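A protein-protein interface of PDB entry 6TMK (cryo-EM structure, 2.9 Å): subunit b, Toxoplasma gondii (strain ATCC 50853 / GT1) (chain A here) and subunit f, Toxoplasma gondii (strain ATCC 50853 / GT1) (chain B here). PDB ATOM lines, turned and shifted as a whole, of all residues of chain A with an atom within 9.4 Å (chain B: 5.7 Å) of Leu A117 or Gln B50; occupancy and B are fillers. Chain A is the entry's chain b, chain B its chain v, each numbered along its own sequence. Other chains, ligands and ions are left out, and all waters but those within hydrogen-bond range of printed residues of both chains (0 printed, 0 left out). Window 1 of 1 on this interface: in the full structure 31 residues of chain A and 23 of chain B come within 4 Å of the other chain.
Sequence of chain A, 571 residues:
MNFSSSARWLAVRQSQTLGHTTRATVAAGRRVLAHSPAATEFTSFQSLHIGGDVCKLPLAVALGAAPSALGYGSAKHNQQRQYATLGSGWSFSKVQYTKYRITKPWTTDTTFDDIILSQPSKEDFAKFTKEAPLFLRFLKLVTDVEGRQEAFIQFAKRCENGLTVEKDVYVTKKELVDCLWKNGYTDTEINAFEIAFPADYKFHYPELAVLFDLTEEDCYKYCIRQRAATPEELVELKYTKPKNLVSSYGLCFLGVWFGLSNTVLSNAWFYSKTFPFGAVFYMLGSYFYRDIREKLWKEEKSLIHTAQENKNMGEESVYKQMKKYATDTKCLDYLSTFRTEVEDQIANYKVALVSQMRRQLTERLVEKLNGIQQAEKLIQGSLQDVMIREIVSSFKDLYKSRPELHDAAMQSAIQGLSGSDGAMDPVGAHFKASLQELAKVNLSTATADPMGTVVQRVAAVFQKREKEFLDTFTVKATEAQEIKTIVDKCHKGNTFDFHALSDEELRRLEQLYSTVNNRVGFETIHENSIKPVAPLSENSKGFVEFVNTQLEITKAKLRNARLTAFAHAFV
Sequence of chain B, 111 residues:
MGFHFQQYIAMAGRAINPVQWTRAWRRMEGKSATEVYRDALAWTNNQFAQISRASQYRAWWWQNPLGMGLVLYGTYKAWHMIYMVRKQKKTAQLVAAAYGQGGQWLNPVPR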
ATOM      1  N   TYR A  83     -23.231  -1.463  -6.611  1.00  0.00           N
ATOM      2  CA  TYR A  83     -23.386  -2.894  -6.822  1.00  0.00           C
ATOM      3  C   TYR A  83     -22.032  -3.570  -6.924  1.00  0.00           C
ATOM      4  O   TYR A  83     -21.048  -2.954  -7.322  1.00  0.00           O
ATOM      5  CB  TYR A  83     -24.209  -3.163  -8.081  1.00  0.00           C
ATOM      6  CG  TYR A  83     -25.670  -2.857  -7.917  1.00  0.00           C
ATOM      7  CD1 TYR A  83     -26.585  -3.865  -7.695  1.00  0.00           C
ATOM      8  CD2 TYR A  83     -26.135  -1.559  -7.977  1.00  0.00           C
ATOM      9  CE1 TYR A  83     -27.917  -3.589  -7.537  1.00  0.00           C
ATOM     10  CE2 TYR A  83     -27.464  -1.277  -7.818  1.00  0.00           C
ATOM     11  CZ  TYR A  83     -28.351  -2.294  -7.597  1.00  0.00           C
ATOM     12  OH  TYR A  83     -29.682  -2.007  -7.440  1.00  0.00           O
ATOM     13  N   ALA A  84     -21.988  -4.845  -6.554  1.00  0.00           N
ATOM     14  CA  ALA A  84     -20.739  -5.586  -6.576  1.00  0.00           C
ATOM     15  C   ALA A  84     -20.305  -5.894  -8.001  1.00  0.00           C
ATOM     16  O   ALA A  84     -21.123  -6.047  -8.911  1.00  0.00           O
ATOM     17  CB  ALA A  84     -20.873  -6.889  -5.798  1.00  0.00           C
ATOM     18  N   PHE A 112     -34.147  -2.336 -25.363  1.00  0.00           N
ATOM     19  CA  PHE A 112     -32.924  -2.849 -24.766  1.00  0.00           C
ATOM     20  C   PHE A 112     -32.388  -1.892 -23.713  1.00  0.00           C
ATOM     21  O   PHE A 112     -32.407  -0.672 -23.900  1.00  0.00           O
ATOM     22  CB  PHE A 112     -31.872  -3.089 -25.837  1.00  0.00           C
ATOM     23  CG  PHE A 112     -32.185  -4.234 -26.734  1.00  0.00           C
ATOM     24  CD1 PHE A 112     -31.571  -5.452 -26.554  1.00  0.00           C
ATOM     25  CD2 PHE A 112     -33.092  -4.093 -27.759  1.00  0.00           C
ATOM     26  CE1 PHE A 112     -31.856  -6.504 -27.376  1.00  0.00           C
ATOM     27  CE2 PHE A 112     -33.380  -5.142 -28.584  1.00  0.00           C
ATOM     28  CZ  PHE A 112     -32.763  -6.348 -28.397  1.00  0.00           C
ATOM     29  N   ASP A 113     -31.908  -2.449 -22.604  1.00  0.00           N
ATOM     30  CA  ASP A 113     -31.433  -1.626 -21.504  1.00  0.00           C
ATOM     31  C   ASP A 113     -30.416  -2.397 -20.678  1.00  0.00           C
ATOM     32  O   ASP A 113     -30.243  -3.607 -20.829  1.00  0.00           O
ATOM     33  CB  ASP A 113     -32.590  -1.165 -20.621  1.00  0.00           C
ATOM     34  CG  ASP A 113     -32.287   0.125 -19.890  1.00  0.00           C
ATOM     35  OD1 ASP A 113     -31.093   0.456 -19.738  1.00  0.00           O
ATOM     36  OD2 ASP A 113     -33.241   0.808 -19.467  1.00  0.00           O
ATOM     37  N   ASP A 114     -29.748  -1.671 -19.787  1.00  0.00           N
ATOM     38  CA  ASP A 114     -28.775  -2.269 -18.887  1.00  0.00           C
ATOM     39  C   ASP A 114     -29.485  -2.870 -17.687  1.00  0.00           C
ATOM     40  O   ASP A 114     -30.401  -2.269 -17.122  1.00  0.00           O
ATOM     41  CB  ASP A 114     -27.761  -1.216 -18.437  1.00  0.00           C
ATOM     42  CG  ASP A 114     -26.592  -1.804 -17.674  1.00  0.00           C
ATOM     43  OD1 ASP A 114     -25.676  -2.352 -18.317  1.00  0.00           O
ATOM     44  OD2 ASP A 114     -26.578  -1.706 -16.432  1.00  0.00           O
ATOM     45  N   ILE A 115     -29.057  -4.069 -17.299  1.00  0.00           N
ATOM     46  CA  ILE A 115     -29.775  -4.800 -16.265  1.00  0.00           C
ATOM     47  C   ILE A 115     -29.635  -4.103 -14.917  1.00  0.00           C
ATOM     48  O   ILE A 115     -30.599  -4.013 -14.147  1.00  0.00           O
ATOM     49  CB  ILE A 115     -29.284  -6.258 -16.229  1.00  0.00           C
ATOM     50  CG1 ILE A 115     -30.155  -7.102 -15.311  1.00  0.00           C
ATOM     51  CG2 ILE A 115     -27.841  -6.344 -15.791  1.00  0.00           C
ATOM     52  CD1 ILE A 115     -29.992  -8.573 -15.548  1.00  0.00           C
ATOM     53  N   ILE A 116     -28.450  -3.567 -14.622  1.00  0.00           N
ATOM     54  CA  ILE A 116     -28.228  -2.956 -13.321  1.00  0.00           C
ATOM     55  C   ILE A 116     -28.918  -1.604 -13.229  1.00  0.00           C
ATOM     56  O   ILE A 116     -29.344  -1.189 -12.145  1.00  0.00           O
ATOM     57  CB  ILE A 116     -26.719  -2.851 -13.053  1.00  0.00           C
ATOM     58  CG1 ILE A 116     -26.163  -4.212 -12.657  1.00  0.00           C
ATOM     59  CG2 ILE A 116     -26.434  -1.844 -11.973  1.00  0.00           C
ATOM     60  CD1 ILE A 116     -24.737  -4.412 -13.025  1.00  0.00           C
ATOM     61  N   LEU A 117     -29.030  -0.890 -14.347  1.00  0.00           N
ATOM     62  CA  LEU A 117     -29.680   0.410 -14.328  1.00  0.00           C
ATOM     63  C   LEU A 117     -31.193   0.282 -14.353  1.00  0.00           C
ATOM     64  O   LEU A 117     -31.890   1.093 -13.735  1.00  0.00           O
ATOM     65  CB  LEU A 117     -29.203   1.244 -15.515  1.00  0.00           C
ATOM     66  CG  LEU A 117     -27.733   1.647 -15.477  1.00  0.00           C
ATOM     67  CD1 LEU A 117     -27.294   2.241 -16.789  1.00  0.00           C
ATOM     68  CD2 LEU A 117     -27.491   2.622 -14.363  1.00  0.00           C
ATOM     69  N   SER A 118     -31.710  -0.720 -15.060  1.00  0.00           N
ATOM     70  CA  SER A 118     -33.145  -0.944 -15.115  1.00  0.00           C
ATOM     71  C   SER A 118     -33.672  -1.569 -13.830  1.00  0.00           C
ATOM     72  O   SER A 118     -34.775  -1.235 -13.385  1.00  0.00           O
ATOM     73  CB  SER A 118     -33.474  -1.830 -16.309  1.00  0.00           C
ATOM     74  OG  SER A 118     -33.426  -1.093 -17.511  1.00  0.00           O
ATOM     75  N   GLN A 119     -32.906  -2.472 -13.227  1.00  0.00           N
ATOM     76  CA  GLN A 119     -33.381  -3.305 -12.130  1.00  0.00           C
ATOM     77  C   GLN A 119     -34.674  -4.023 -12.523  1.00  0.00           C
ATOM     78  O   GLN A 119     -35.699  -3.885 -11.849  1.00  0.00           O
ATOM     79  CB  GLN A 119     -33.586  -2.475 -10.870  1.00  0.00           C
ATOM     80  CG  GLN A 119     -32.305  -1.950 -10.260  1.00  0.00           C
ATOM     81  CD  GLN A 119     -31.449  -3.057  -9.698  1.00  0.00           C
ATOM     82  OE1 GLN A 119     -31.913  -3.871  -8.901  1.00  0.00           O
ATOM     83  NE2 GLN A 119     -30.194  -3.101 -10.115  1.00  0.00           N
ATOM     84  N   PRO A 120     -34.656  -4.793 -13.606  1.00  0.00           N
ATOM     85  CA  PRO A 120     -35.903  -5.337 -14.139  1.00  0.00           C
ATOM     86  C   PRO A 120     -36.448  -6.483 -13.309  1.00  0.00           C
ATOM     87  O   PRO A 120     -35.714  -7.202 -12.629  1.00  0.00           O
ATOM     88  CB  PRO A 120     -35.501  -5.813 -15.534  1.00  0.00           C
ATOM     89  CG  PRO A 120     -34.103  -6.211 -15.371  1.00  0.00           C
ATOM     90  CD  PRO A 120     -33.501  -5.234 -14.401  1.00  0.00           C
ATOM     91  N   ALA A 228     -25.521 -10.706 -14.975  1.00  0.00           N
ATOM     92  CA  ALA A 228     -24.951  -9.511 -14.368  1.00  0.00           C
ATOM     93  C   ALA A 228     -23.433  -9.564 -14.335  1.00  0.00           C
ATOM     94  O   ALA A 228     -22.780  -8.516 -14.308  1.00  0.00           O
ATOM     95  CB  ALA A 228     -25.501  -9.338 -12.958  1.00  0.00           C
ATOM     96  N   PRO A 231     -22.474  -7.560 -17.775  1.00  0.00           N
ATOM     97  CA  PRO A 231     -23.524  -6.561 -17.980  1.00  0.00           C
ATOM     98  C   PRO A 231     -23.297  -5.622 -19.152  1.00  0.00           C
ATOM     99  O   PRO A 231     -24.135  -4.747 -19.390  1.00  0.00           O
ATOM    100  CB  PRO A 231     -23.492  -5.801 -16.652  1.00  0.00           C
ATOM    101  CG  PRO A 231     -22.088  -5.977 -16.127  1.00  0.00           C
ATOM    102  CD  PRO A 231     -21.391  -7.013 -16.949  1.00  0.00           C
ATOM    103  N   LEU A 234     -26.637  -5.765 -23.308  1.00  0.00           N
ATOM    104  CA  LEU A 234     -27.946  -5.251 -22.947  1.00  0.00           C
ATOM    105  C   LEU A 234     -28.976  -6.370 -22.938  1.00  0.00           C
ATOM    106  O   LEU A 234     -28.826  -7.395 -23.606  1.00  0.00           O
ATOM    107  CB  LEU A 234     -28.373  -4.158 -23.916  1.00  0.00           C
ATOM    108  CG  LEU A 234     -27.421  -2.978 -24.074  1.00  0.00           C
ATOM    109  CD1 LEU A 234     -27.962  -2.045 -25.108  1.00  0.00           C
ATOM    110  CD2 LEU A 234     -27.224  -2.242 -22.769  1.00  0.00           C
ATOM    111  N   VAL A 235     -30.029  -6.165 -22.158  1.00  0.00           N
ATOM    112  CA  VAL A 235     -31.098  -7.139 -22.015  1.00  0.00           C
ATOM    113  C   VAL A 235     -32.383  -6.532 -22.547  1.00  0.00           C
ATOM    114  O   VAL A 235     -32.575  -5.311 -22.537  1.00  0.00           O
ATOM    115  CB  VAL A 235     -31.275  -7.606 -20.553  1.00  0.00           C
ATOM    116  CG1 VAL A 235     -29.969  -8.078 -19.991  1.00  0.00           C
ATOM    117  CG2 VAL A 235     -31.830  -6.501 -19.699  1.00  0.00           C
ATOM    118  N   LEU A 237     -36.327  -5.869 -22.685  1.00  0.00           N
ATOM    119  CA  LEU A 237     -37.427  -5.614 -21.778  1.00  0.00           C
ATOM    120  C   LEU A 237     -38.668  -5.281 -22.587  1.00  0.00           C
ATOM    121  O   LEU A 237     -38.591  -4.939 -23.768  1.00  0.00           O
ATOM    122  CB  LEU A 237     -37.111  -4.457 -20.833  1.00  0.00           C
ATOM    123  CG  LEU A 237     -36.347  -4.737 -19.549  1.00  0.00           C
ATOM    124  CD1 LEU A 237     -34.917  -4.954 -19.851  1.00  0.00           C
ATOM    125  CD2 LEU A 237     -36.500  -3.563 -18.615  1.00  0.00           C
ATOM    126  N   PHE B   3     -27.534  10.077 -13.810  1.00  0.00           N
ATOM    127  CA  PHE B   3     -28.399   9.311 -14.694  1.00  0.00           C
ATOM    128  C   PHE B   3     -29.837   9.462 -14.226  1.00  0.00           C
ATOM    129  O   PHE B   3     -30.101   9.807 -13.072  1.00  0.00           O
ATOM    130  CB  PHE B   3     -27.991   7.836 -14.725  1.00  0.00           C
ATOM    131  CG  PHE B   3     -28.277   7.102 -13.456  1.00  0.00           C
ATOM    132  CD1 PHE B   3     -27.548   7.341 -12.316  1.00  0.00           C
ATOM    133  CD2 PHE B   3     -29.250   6.132 -13.423  1.00  0.00           C
ATOM    134  CE1 PHE B   3     -27.819   6.657 -11.158  1.00  0.00           C
ATOM    135  CE2 PHE B   3     -29.520   5.446 -12.269  1.00  0.00           C
ATOM    136  CZ  PHE B   3     -28.799   5.705 -11.137  1.00  0.00           C
ATOM    137  N   HIS B   4     -30.761   9.204 -15.149  1.00  0.00           N
ATOM    138  CA  HIS B   4     -32.199   9.148 -14.870  1.00  0.00           C
ATOM    139  C   HIS B   4     -32.778  10.510 -14.488  1.00  0.00           C
ATOM    140  O   HIS B   4     -33.670  10.614 -13.641  1.00  0.00           O
ATOM    141  CB  HIS B   4     -32.473   8.119 -13.780  1.00  0.00           C
ATOM    142  CG  HIS B   4     -32.272   6.707 -14.227  1.00  0.00           C
ATOM    143  ND1 HIS B   4     -32.246   5.646 -13.350  1.00  0.00           N
ATOM    144  CD2 HIS B   4     -32.061   6.185 -15.456  1.00  0.00           C
ATOM    145  CE1 HIS B   4     -32.035   4.529 -14.022  1.00  0.00           C
ATOM    146  NE2 HIS B   4     -31.921   4.829 -15.302  1.00  0.00           N
ATOM    147  N   ASN B  45     -28.740   5.572  -2.063  1.00  0.00           N
ATOM    148  CA  ASN B  45     -27.606   4.667  -2.171  1.00  0.00           C
ATOM    149  C   ASN B  45     -27.680   3.831  -3.438  1.00  0.00           C
ATOM    150  O   ASN B  45     -26.660   3.579  -4.077  1.00  0.00           O
ATOM    151  CB  ASN B  45     -27.526   3.762  -0.950  1.00  0.00           C
ATOM    152  CG  ASN B  45     -26.293   2.898  -0.963  1.00  0.00           C
ATOM    153  OD1 ASN B  45     -25.186   3.378  -0.741  1.00  0.00           O
ATOM    154  ND2 ASN B  45     -26.471   1.620  -1.248  1.00  0.00           N
ATOM    155  N   ASN B  46     -28.876   3.377  -3.806  1.00  0.00           N
ATOM    156  CA  ASN B  46     -29.019   2.576  -5.013  1.00  0.00           C
ATOM    157  C   ASN B  46     -28.633   3.382  -6.238  1.00  0.00           C
ATOM    158  O   ASN B  46     -27.970   2.871  -7.146  1.00  0.00           O
ATOM    159  CB  ASN B  46     -30.450   2.059  -5.128  1.00  0.00           C
ATOM    160  CG  ASN B  46     -30.599   0.978  -6.175  1.00  0.00           C
ATOM    161  OD1 ASN B  46     -29.741   0.108  -6.312  1.00  0.00           O
ATOM    162  ND2 ASN B  46     -31.695   1.025  -6.919  1.00  0.00           N
ATOM    163  N   GLN B  47     -29.010   4.657  -6.265  1.00  0.00           N
ATOM    164  CA  GLN B  47     -28.625   5.508  -7.384  1.00  0.00           C
ATOM    165  C   GLN B  47     -27.111   5.647  -7.471  1.00  0.00           C
ATOM    166  O   GLN B  47     -26.499   5.407  -8.526  1.00  0.00           O
ATOM    167  CB  GLN B  47     -29.273   6.883  -7.240  1.00  0.00           C
ATOM    168  CG  GLN B  47     -30.776   6.889  -7.260  1.00  0.00           C
ATOM    169  CD  GLN B  47     -31.344   6.458  -8.585  1.00  0.00           C
ATOM    170  OE1 GLN B  47     -31.090   7.077  -9.615  1.00  0.00           O
ATOM    171  NE2 GLN B  47     -32.134   5.405  -8.565  1.00  0.00           N
ATOM    172  N   PHE B  48     -26.482   6.037  -6.362  1.00  0.00           N
ATOM    173  CA  PHE B  48     -25.041   6.253  -6.404  1.00  0.00           C
ATOM    174  C   PHE B  48     -24.280   4.957  -6.657  1.00  0.00           C
ATOM    175  O   PHE B  48     -23.221   4.973  -7.296  1.00  0.00           O
ATOM    176  CB  PHE B  48     -24.581   6.910  -5.108  1.00  0.00           C
ATOM    177  CG  PHE B  48     -24.919   8.361  -5.023  1.00  0.00           C
ATOM    178  CD1 PHE B  48     -24.304   9.280  -5.844  1.00  0.00           C
ATOM    179  CD2 PHE B  48     -25.853   8.810  -4.117  1.00  0.00           C
ATOM    180  CE1 PHE B  48     -24.621  10.612  -5.765  1.00  0.00           C
ATOM    181  CE2 PHE B  48     -26.171  10.138  -4.036  1.00  0.00           C
ATOM    182  CZ  PHE B  48     -25.555  11.040  -4.857  1.00  0.00           C
ATOM    183  N   ALA B  49     -24.807   3.825  -6.190  1.00  0.00           N
ATOM    184  CA  ALA B  49     -24.170   2.542  -6.443  1.00  0.00           C
ATOM    185  C   ALA B  49     -24.309   2.127  -7.901  1.00  0.00           C
ATOM    186  O   ALA B  49     -23.382   1.544  -8.475  1.00  0.00           O
ATOM    187  CB  ALA B  49     -24.767   1.490  -5.517  1.00  0.00           C
ATOM    188  N   GLN B  50     -25.460   2.410  -8.516  1.00  0.00           N
ATOM    189  CA  GLN B  50     -25.590   2.203  -9.951  1.00  0.00           C
ATOM    190  C   GLN B  50     -24.528   2.981 -10.700  1.00  0.00           C
ATOM    191  O   GLN B  50     -23.905   2.462 -11.629  1.00  0.00           O
ATOM    192  CB  GLN B  50     -26.965   2.643 -10.440  1.00  0.00           C
ATOM    193  CG  GLN B  50     -28.096   1.702 -10.197  1.00  0.00           C
ATOM    194  CD  GLN B  50     -29.410   2.303 -10.625  1.00  0.00           C
ATOM    195  OE1 GLN B  50     -29.618   2.586 -11.800  1.00  0.00           O
ATOM    196  NE2 GLN B  50     -30.300   2.518  -9.675  1.00  0.00           N
ATOM    197  N   ILE B  51     -24.300   4.230 -10.300  1.00  0.00           N
ATOM    198  CA  ILE B  51     -23.251   5.018 -10.941  1.00  0.00           C
ATOM    199  C   ILE B  51     -21.898   4.341 -10.761  1.00  0.00           C
ATOM    200  O   ILE B  51     -21.177   4.079 -11.733  1.00  0.00           O
ATOM    201  CB  ILE B  51     -23.242   6.456 -10.399  1.00  0.00           C
ATOM    202  CG1 ILE B  51     -24.553   7.148 -10.752  1.00  0.00           C
ATOM    203  CG2 ILE B  51     -22.069   7.225 -10.958  1.00  0.00           C
ATOM    204  CD1 ILE B  51     -24.762   8.450 -10.057  1.00  0.00           C
ATOM    205  N   SER B  52     -21.536   4.053  -9.512  1.00  0.00           N
ATOM    206  CA  SER B  52     -20.207   3.529  -9.224  1.00  0.00           C
ATOM    207  C   SER B  52     -19.944   2.229  -9.971  1.00  0.00           C
ATOM    208  O   SER B  52     -18.815   1.971 -10.401  1.00  0.00           O
ATOM    209  CB  SER B  52     -20.041   3.316  -7.721  1.00  0.00           C
ATOM    210  OG  SER B  52     -20.285   4.507  -6.998  1.00  0.00           O
ATOM    211  N   ARG B  53     -20.971   1.400 -10.143  1.00  0.00           N
ATOM    212  CA  ARG B  53     -20.789   0.142 -10.851  1.00  0.00           C
ATOM    213  C   ARG B  53     -20.765   0.337 -12.363  1.00  0.00           C
ATOM    214  O   ARG B  53     -19.854  -0.151 -13.039  1.00  0.00           O
ATOM    215  CB  ARG B  53     -21.901  -0.822 -10.449  1.00  0.00           C
ATOM    216  CG  ARG B  53     -21.898  -2.154 -11.158  1.00  0.00           C
ATOM    217  CD  ARG B  53     -20.579  -2.863 -11.062  1.00  0.00           C
ATOM    218  NE  ARG B  53     -20.693  -4.221 -11.572  1.00  0.00           N
ATOM    219  CZ  ARG B  53     -19.927  -4.748 -12.521  1.00  0.00           C
ATOM    220  NH1 ARG B  53     -20.131  -5.996 -12.902  1.00  0.00           N
ATOM    221  NH2 ARG B  53     -18.957  -4.050 -13.085  1.00  0.00           N
ATOM    222  N   ALA B  54     -21.750   1.042 -12.916  1.00  0.00           N
ATOM    223  CA  ALA B  54     -21.924   1.083 -14.360  1.00  0.00           C
ATOM    224  C   ALA B  54     -20.931   2.006 -15.051  1.00  0.00           C
ATOM    225  O   ALA B  54     -20.729   1.871 -16.260  1.00  0.00           O
ATOM    226  CB  ALA B  54     -23.354   1.485 -14.715  1.00  0.00           C
ATOM    227  N   SER B  55     -20.309   2.935 -14.324  1.00  0.00           N
ATOM    228  CA  SER B  55     -19.296   3.780 -14.940  1.00  0.00           C
ATOM    229  C   SER B  55     -18.059   2.994 -15.340  1.00  0.00           C
ATOM    230  O   SER B  55     -17.283   3.463 -16.177  1.00  0.00           O
ATOM    231  CB  SER B  55     -18.897   4.900 -13.986  1.00  0.00           C
ATOM    232  OG  SER B  55     -20.031   5.551 -13.455  1.00  0.00           O
ATOM    233  N   ARG B  58     -19.691   1.181 -18.885  1.00  0.00           N
ATOM    234  CA  ARG B  58     -20.718   1.769 -19.724  1.00  0.00           C
ATOM    235  C   ARG B  58     -20.516   3.271 -19.866  1.00  0.00           C
ATOM    236  O   ARG B  58     -19.982   3.934 -18.974  1.00  0.00           O
ATOM    237  CB  ARG B  58     -22.101   1.498 -19.151  1.00  0.00           C
ATOM    238  CG  ARG B  58     -23.212   1.930 -20.046  1.00  0.00           C
ATOM    239  CD  ARG B  58     -24.418   1.020 -20.000  1.00  0.00           C
ATOM    240  NE  ARG B  58     -24.161  -0.378 -20.327  1.00  0.00           N
ATOM    241  CZ  ARG B  58     -23.756  -0.807 -21.513  1.00  0.00           C
ATOM    242  NH1 ARG B  58     -23.543   0.038 -22.496  1.00  0.00           N
ATOM    243  NH2 ARG B  58     -23.567  -2.093 -21.715  1.00  0.00           N
ATOM    244  N   TRP B  60     -22.635   6.853 -21.188  1.00  0.00           N
ATOM    245  CA  TRP B  60     -23.898   7.463 -21.552  1.00  0.00           C
ATOM    246  C   TRP B  60     -23.742   8.330 -22.797  1.00  0.00           C
ATOM    247  O   TRP B  60     -22.639   8.596 -23.275  1.00  0.00           O
ATOM    248  CB  TRP B  60     -24.430   8.298 -20.396  1.00  0.00           C
ATOM    249  CG  TRP B  60     -24.993   7.505 -19.269  1.00  0.00           C
ATOM    250  CD1 TRP B  60     -26.302   7.235 -19.037  1.00  0.00           C
ATOM    251  CD2 TRP B  60     -24.264   6.893 -18.202  1.00  0.00           C
ATOM    252  NE1 TRP B  60     -26.438   6.488 -17.901  1.00  0.00           N
ATOM    253  CE2 TRP B  60     -25.200   6.265 -17.367  1.00  0.00           C
ATOM    254  CE3 TRP B  60     -22.912   6.815 -17.872  1.00  0.00           C
ATOM    255  CZ2 TRP B  60     -24.828   5.564 -16.228  1.00  0.00           C
ATOM    256  CZ3 TRP B  60     -22.548   6.121 -16.742  1.00  0.00           C
ATOM    257  CH2 TRP B  60     -23.500   5.506 -15.935  1.00  0.00           C
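The guanidinium group (NE) of Arg B53 sits at hydrogen-bond distance from the backbone carbonyl oxygen (O) of Ala A84 (3.3 Å).
The side-chain amide oxygen (OE1) of Gln B50 lies close to the backbone carbonyl oxygen (O) of Leu A117, at 3.3 Å.
OD1 of Asn B46 sits close to OH of Tyr A83 (2.4 Å).
The side-chain carboxylate (OD1) of Asp A114 lies within salt-bridge range of the guanidinium group (NE) of Arg B58 (3.2 Å).
Among the printed residues, pairs that only touch across the chains: Tyr A83 with Ala B49 (3.5 Å), Tyr A83 with Gln B50 (3.9 Å), Tyr A83 with Arg B53 (3.8 Å), Ile A116 with Gln B50 (3.7 Å), Leu A117 with His B4 (3.5 Å), Ala A228 with Arg B53 (3.9 Å), Pro A231 with Arg B53 (3.8 Å), Pro A231 with Arg B58 (3.6 Å) and Leu A234 with Arg B58 (3.8 Å).
The side-chain amide nitrogen of Gln B50 lies close to the side-chain amide nitrogen of Asn B46, 3.4 Å away.
O of Ile A116 is in hydrogen-bond range of NE2 of Gln A119 (2.9 Å).
NE2 of Gln A119 is in hydrogen-bond range of OH of Tyr A83 (2.9 Å).
O of Asp A114 lies close to OG of Ser A118 (3.3 Å).
The side-chain carboxylate (OD2) of Asp A114 is in hydrogen-bond range of the backbone NH (N) of Leu A117 (3.3 Å).
N of Ile A116 is in hydrogen-bond range of OD2 of Asp A114 (3.2 Å).
Of the 15 printed residues of chain B, 6 touch a printed residue of chain A.
Printed residues of chain B that touch a printed residue of chain A: His B4, Asn B46, Ala B49, Gln B50, Arg B53 and Arg B58.
Hydrophobic or aromatic side chains of chain B within 4 Å of the printed part of chain A: His B4 and Ala B49.
Of the 16 printed residues of chain A, 8 touch a printed residue of chain B.
Hydrophobic or aromatic side chains of chain A within 4 Å of the printed part of chain B: Tyr A83, Leu A117, Pro A231 and Leu A234.
Among the printed residues, 13 pairs touch across the chains.
Printed residues of chain B within 4 Å of Tyr A83: Asn B46, Ala B49, Gln B50 and Arg B53.
Of the printed residues of chain B, Ala A84 touches Arg B53.
Ile A115 touches none of the printed residues of chain B.
Printed residues of chain A within 4 Å of His B4: Leu A117.
Phe B48 touches none of the printed residues of chain A.
Ala B49 touches one residue of chain A.
Gln B50 touches just these residues of chain A: Tyr A83, Ile A116 and Leu A117.
Of the printed residues of chain A, Arg B53 touches Tyr A83, Ala A84, Ala A228 and Pro A231.
Printed residues of chain A within 4 Å of Arg B58: Asp A114 (3.2 Å), Pro A231 (3.6 Å) and Leu A234 (3.8 Å).
The nearest residue of chain B that does not touch Leu A117 is Phe B3 (4.04 Å).
The nearest residue of chain A that does not touch Gln B50 is Gln A119 (4.9 Å).
The nearest printed residue of chain B that does not touch Ala A84 is Ala B49 (6.8 Å).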
